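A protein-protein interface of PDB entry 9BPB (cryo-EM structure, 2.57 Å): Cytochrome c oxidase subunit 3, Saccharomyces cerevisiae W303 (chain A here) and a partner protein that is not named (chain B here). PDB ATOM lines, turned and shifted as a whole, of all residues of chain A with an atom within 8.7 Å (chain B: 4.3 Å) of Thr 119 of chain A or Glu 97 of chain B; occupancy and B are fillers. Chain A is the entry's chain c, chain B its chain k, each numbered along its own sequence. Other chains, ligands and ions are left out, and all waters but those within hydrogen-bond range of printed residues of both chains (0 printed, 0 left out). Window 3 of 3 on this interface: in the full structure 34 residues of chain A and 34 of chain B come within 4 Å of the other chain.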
ATOM      1  N   PRO A 116      20.781 -26.873  -8.670  1.00  0.00           N
ATOM      2  CA  PRO A 116      21.885 -26.381  -7.836  1.00  0.00           C
ATOM      3  C   PRO A 116      21.704 -24.918  -7.460  1.00  0.00           C
ATOM      4  O   PRO A 116      21.169 -24.119  -8.230  1.00  0.00           O
ATOM      5  CB  PRO A 116      23.119 -26.588  -8.720  1.00  0.00           C
ATOM      6  CG  PRO A 116      22.589 -26.655 -10.111  1.00  0.00           C
ATOM      7  CD  PRO A 116      21.236 -27.281 -10.010  1.00  0.00           C
ATOM      8  N   ASP A 117      22.156 -24.578  -6.256  1.00  0.00           N
ATOM      9  CA  ASP A 117      21.964 -23.243  -5.713  1.00  0.00           C
ATOM     10  C   ASP A 117      22.764 -22.215  -6.507  1.00  0.00           C
ATOM     11  O   ASP A 117      23.700 -22.539  -7.240  1.00  0.00           O
ATOM     12  CB  ASP A 117      22.369 -23.211  -4.238  1.00  0.00           C
ATOM     13  CG  ASP A 117      21.836 -21.991  -3.508  1.00  0.00           C
ATOM     14  OD1 ASP A 117      22.080 -20.857  -3.968  1.00  0.00           O
ATOM     15  OD2 ASP A 117      21.166 -22.170  -2.469  1.00  0.00           O
ATOM     16  N   VAL A 118      22.371 -20.948  -6.348  1.00  0.00           N
ATOM     17  CA  VAL A 118      22.995 -19.868  -7.102  1.00  0.00           C
ATOM     18  C   VAL A 118      24.278 -19.393  -6.430  1.00  0.00           C
ATOM     19  O   VAL A 118      25.176 -18.864  -7.097  1.00  0.00           O
ATOM     20  CB  VAL A 118      21.990 -18.716  -7.285  1.00  0.00           C
ATOM     21  CG1 VAL A 118      22.523 -17.698  -8.261  1.00  0.00           C
ATOM     22  CG2 VAL A 118      20.654 -19.259  -7.760  1.00  0.00           C
ATOM     23  N   THR A 119      24.387 -19.554  -5.108  1.00  0.00           N
ATOM     24  CA  THR A 119      25.639 -19.226  -4.430  1.00  0.00           C
ATOM     25  C   THR A 119      26.737 -20.205  -4.824  1.00  0.00           C
ATOM     26  O   THR A 119      27.925 -19.864  -4.805  1.00  0.00           O
ATOM     27  CB  THR A 119      25.438 -19.219  -2.917  1.00  0.00           C
ATOM     28  OG1 THR A 119      25.378 -20.566  -2.438  1.00  0.00           O
ATOM     29  CG2 THR A 119      24.149 -18.502  -2.563  1.00  0.00           C
ATOM     30  N   LEU A 120      26.354 -21.428  -5.180  1.00  0.00           N
ATOM     31  CA  LEU A 120      27.253 -22.329  -5.877  1.00  0.00           C
ATOM     32  C   LEU A 120      27.379 -21.874  -7.328  1.00  0.00           C
ATOM     33  O   LEU A 120      26.878 -20.819  -7.726  1.00  0.00           O
ATOM     34  CB  LEU A 120      26.734 -23.762  -5.811  1.00  0.00           C
ATOM     35  CG  LEU A 120      26.476 -24.396  -4.444  1.00  0.00           C
ATOM     36  CD1 LEU A 120      25.815 -25.748  -4.622  1.00  0.00           C
ATOM     37  CD2 LEU A 120      27.758 -24.529  -3.650  1.00  0.00           C
ATOM     38  N   GLY A 121      28.046 -22.674  -8.140  1.00  0.00           N
ATOM     39  CA  GLY A 121      27.993 -22.438  -9.564  1.00  0.00           C
ATOM     40  C   GLY A 121      26.617 -22.760 -10.111  1.00  0.00           C
ATOM     41  O   GLY A 121      25.731 -23.261  -9.417  1.00  0.00           O
ATOM     42  N   ALA A 122      26.430 -22.465 -11.395  1.00  0.00           N
ATOM     43  CA  ALA A 122      25.212 -22.902 -12.059  1.00  0.00           C
ATOM     44  C   ALA A 122      25.189 -24.406 -12.291  1.00  0.00           C
ATOM     45  O   ALA A 122      24.192 -24.924 -12.804  1.00  0.00           O
ATOM     46  CB  ALA A 122      25.044 -22.170 -13.392  1.00  0.00           C
ATOM     47  N   CYS A 123      26.259 -25.109 -11.926  1.00  0.00           N
ATOM     48  CA  CYS A 123      26.433 -26.522 -12.209  1.00  0.00           C
ATOM     49  C   CYS A 123      26.455 -27.333 -10.913  1.00  0.00           C
ATOM     50  O   CYS A 123      26.272 -26.813  -9.811  1.00  0.00           O
ATOM     51  CB  CYS A 123      27.721 -26.740 -13.007  1.00  0.00           C
ATOM     52  SG  CYS A 123      27.771 -25.888 -14.602  1.00  0.00           S
ATOM     53  N   PRO A 126      29.820 -28.263  -7.409  1.00  0.00           N
ATOM     54  CA  PRO A 126      30.134 -26.829  -7.468  1.00  0.00           C
ATOM     55  C   PRO A 126      31.480 -26.559  -8.121  1.00  0.00           C
ATOM     56  O   PRO A 126      32.312 -27.451  -8.300  1.00  0.00           O
ATOM     57  CB  PRO A 126      30.138 -26.405  -5.996  1.00  0.00           C
ATOM     58  CG  PRO A 126      29.292 -27.419  -5.309  1.00  0.00           C
ATOM     59  CD  PRO A 126      29.534 -28.703  -6.033  1.00  0.00           C
ATOM     60  N   VAL A 127      31.686 -25.291  -8.476  1.00  0.00           N
ATOM     61  CA  VAL A 127      32.891 -24.895  -9.192  1.00  0.00           C
ATOM     62  C   VAL A 127      34.092 -24.998  -8.264  1.00  0.00           C
ATOM     63  O   VAL A 127      34.085 -24.461  -7.148  1.00  0.00           O
ATOM     64  CB  VAL A 127      32.740 -23.471  -9.747  1.00  0.00           C
ATOM     65  CG1 VAL A 127      34.016 -23.038 -10.442  1.00  0.00           C
ATOM     66  CG2 VAL A 127      31.560 -23.393 -10.700  1.00  0.00           C
ATOM     67  N   SER A 197      33.689 -28.846   5.500  1.00  0.00           N
ATOM     68  CA  SER A 197      33.391 -27.423   5.562  1.00  0.00           C
ATOM     69  C   SER A 197      33.279 -26.782   4.185  1.00  0.00           C
ATOM     70  O   SER A 197      33.135 -25.560   4.097  1.00  0.00           O
ATOM     71  CB  SER A 197      34.465 -26.702   6.381  1.00  0.00           C
ATOM     72  OG  SER A 197      34.519 -27.195   7.706  1.00  0.00           O
ATOM     73  N   ASP A 198      33.338 -27.573   3.115  1.00  0.00           N
ATOM     74  CA  ASP A 198      33.354 -27.030   1.756  1.00  0.00           C
ATOM     75  C   ASP A 198      31.934 -26.864   1.213  1.00  0.00           C
ATOM     76  O   ASP A 198      31.504 -27.535   0.276  1.00  0.00           O
ATOM     77  CB  ASP A 198      34.197 -27.914   0.846  1.00  0.00           C
ATOM     78  CG  ASP A 198      35.676 -27.594   0.934  1.00  0.00           C
ATOM     79  OD1 ASP A 198      36.069 -26.847   1.851  1.00  0.00           O
ATOM     80  OD2 ASP A 198      36.444 -28.076   0.079  1.00  0.00           O
ATOM     81  N   GLY A 199      31.205 -25.933   1.822  1.00  0.00           N
ATOM     82  CA  GLY A 199      29.874 -25.630   1.344  1.00  0.00           C
ATOM     83  C   GLY A 199      28.893 -26.769   1.571  1.00  0.00           C
ATOM     84  O   GLY A 199      29.048 -27.607   2.462  1.00  0.00           O
ATOM     85  N   VAL A 200      27.861 -26.787   0.727  1.00  0.00           N
ATOM     86  CA  VAL A 200      26.816 -27.795   0.858  1.00  0.00           C
ATOM     87  C   VAL A 200      27.244 -29.122   0.235  1.00  0.00           C
ATOM     88  O   VAL A 200      26.763 -30.184   0.647  1.00  0.00           O
ATOM     89  CB  VAL A 200      25.504 -27.279   0.240  1.00  0.00           C
ATOM     90  CG1 VAL A 200      25.646 -27.111  -1.260  1.00  0.00           C
ATOM     91  CG2 VAL A 200      24.347 -28.207   0.576  1.00  0.00           C
ATOM     92  N   ASP B  95      39.750 -19.251  -2.651  1.00  0.00           N
ATOM     93  CA  ASP B  95      38.563 -19.953  -2.185  1.00  0.00           C
ATOM     94  C   ASP B  95      37.310 -19.154  -2.520  1.00  0.00           C
ATOM     95  O   ASP B  95      37.268 -17.938  -2.314  1.00  0.00           O
ATOM     96  CB  ASP B  95      38.642 -20.196  -0.678  1.00  0.00           C
ATOM     97  CG  ASP B  95      39.822 -21.059  -0.290  1.00  0.00           C
ATOM     98  OD1 ASP B  95      40.230 -21.911  -1.106  1.00  0.00           O
ATOM     99  OD2 ASP B  95      40.339 -20.890   0.832  1.00  0.00           O
ATOM    100  N   TYR B  96      36.295 -19.846  -3.029  1.00  0.00           N
ATOM    101  CA  TYR B  96      35.011 -19.217  -3.284  1.00  0.00           C
ATOM    102  C   TYR B  96      34.318 -18.887  -1.963  1.00  0.00           C
ATOM    103  O   TYR B  96      34.758 -19.279  -0.879  1.00  0.00           O
ATOM    104  CB  TYR B  96      34.133 -20.126  -4.142  1.00  0.00           C
ATOM    105  CG  TYR B  96      34.578 -20.223  -5.583  1.00  0.00           C
ATOM    106  CD1 TYR B  96      35.618 -21.062  -5.953  1.00  0.00           C
ATOM    107  CD2 TYR B  96      33.962 -19.471  -6.570  1.00  0.00           C
ATOM    108  CE1 TYR B  96      36.031 -21.152  -7.264  1.00  0.00           C
ATOM    109  CE2 TYR B  96      34.368 -19.552  -7.886  1.00  0.00           C
ATOM    110  CZ  TYR B  96      35.401 -20.393  -8.228  1.00  0.00           C
ATOM    111  OH  TYR B  96      35.806 -20.476  -9.538  1.00  0.00           O
ATOM    112  N   GLU B  97      33.212 -18.146  -2.064  1.00  0.00           N
ATOM    113  CA  GLU B  97      32.532 -17.667  -0.867  1.00  0.00           C
ATOM    114  C   GLU B  97      31.990 -18.803  -0.009  1.00  0.00           C
ATOM    115  O   GLU B  97      31.720 -18.591   1.178  1.00  0.00           O
ATOM    116  CB  GLU B  97      31.397 -16.711  -1.248  1.00  0.00           C
ATOM    117  CG  GLU B  97      30.304 -17.323  -2.113  1.00  0.00           C
ATOM    118  CD  GLU B  97      30.628 -17.292  -3.598  1.00  0.00           C
ATOM    119  OE1 GLU B  97      31.806 -17.072  -3.952  1.00  0.00           O
ATOM    120  OE2 GLU B  97      29.701 -17.485  -4.412  1.00  0.00           O
ATOM    121  N   PHE B  98      31.826 -19.997  -0.573  1.00  0.00           N
ATOM    122  CA  PHE B  98      31.300 -21.138   0.160  1.00  0.00           C
ATOM    123  C   PHE B  98      32.370 -22.148   0.542  1.00  0.00           C
ATOM    124  O   PHE B  98      32.031 -23.242   1.003  1.00  0.00           O
ATOM    125  CB  PHE B  98      30.214 -21.843  -0.662  1.00  0.00           C
ATOM    126  CG  PHE B  98      30.614 -22.147  -2.081  1.00  0.00           C
ATOM    127  CD1 PHE B  98      31.210 -23.354  -2.400  1.00  0.00           C
ATOM    128  CD2 PHE B  98      30.373 -21.241  -3.097  1.00  0.00           C
ATOM    129  CE1 PHE B  98      31.574 -23.644  -3.701  1.00  0.00           C
ATOM    130  CE2 PHE B  98      30.733 -21.524  -4.400  1.00  0.00           C
ATOM    131  CZ  PHE B  98      31.335 -22.728  -4.700  1.00  0.00           C
ATOM    132  N   MET B  99      33.650 -21.813   0.378  1.00  0.00           N
ATOM    133  CA  MET B  99      34.687 -22.839   0.403  1.00  0.00           C
ATOM    134  C   MET B  99      35.024 -23.265   1.827  1.00  0.00           C
ATOM    135  O   MET B  99      34.862 -24.434   2.188  1.00  0.00           O
ATOM    136  CB  MET B  99      35.931 -22.342  -0.327  1.00  0.00           C
ATOM    137  CG  MET B  99      36.879 -23.449  -0.745  1.00  0.00           C
ATOM    138  SD  MET B  99      36.161 -24.541  -1.984  1.00  0.00           S
ATOM    139  CE  MET B  99      36.216 -23.495  -3.432  1.00  0.00           C
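Printed residues of chain B that touch a printed residue of chain A: Tyr 96, Glu 97, Phe 98 and Met 99. Hydrophobic or aromatic side chains of chain B that line the printed part of chain A: Tyr 96 and Phe 98. Printed residues of chain A that touch a printed residue of chain B: Thr 119, Leu 120, Pro 126, Val 127, Ser 197, Asp 198 and Gly 199. Hydrophobic or aromatic side chains of chain A that line the printed part of chain B: Leu 120, Pro 126 and Val 127. Along chain A the printed residues that touch a printed residue of chain B span positions 119 to 199.
The side-chain carboxylate (OD1) of Asp 117 of chain A sits at hydrogen-bond distance from the backbone NH (N) of Thr 119 of chain A, 2.9 Å away.
Among the printed residues, merely in contact across the chains: Thr 119 of chain A with Phe 98 of chain B, Leu 120 of chain A with Phe 98 of chain B, Pro 126 of chain A with Phe 98 of chain B, Val 127 of chain A with Tyr 96 of chain B, Asp 198 of chain A with Phe 98 of chain B and Gly 199 of chain A with Met 99 of chain B.
N of Gly 199 of chain A sits at hydrogen-bond distance from O of Phe 98 of chain B. The side-chain carboxylate (OE2) of Glu 97 of chain B sits close to the backbone carbonyl oxygen (O) of Thr 119 of chain A (3.0 Å). The backbone carbonyl oxygen (O) of Ser 197 of chain A sits close to the backbone carbonyl oxygen (O) of Met 99 of chain B (2.8 Å). The backbone carbonyl oxygen (O) of Met 99 of chain B lies close to the side-chain carboxylate (OD1) of Asp 198 of chain A (2.7 Å).
Printed residues of chain B within 4 Å of Gly 199 of chain A: Phe 98 and Met 99. Printed residues of chain B within 4 Å of Ser 197 of chain A: Met 99 (2.8 Å). Of the printed residues of chain B, Asp 198 of chain A touches Phe 98 (3.6 Å) and Met 99 (2.7 Å). The nearest printed residue of chain B that does not touch Thr 119 of chain A is Tyr 96 of chain B (6.2 Å). The nearest residue of chain A that does not touch Glu 97 of chain B is Leu 120 of chain A (5.2 Å).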
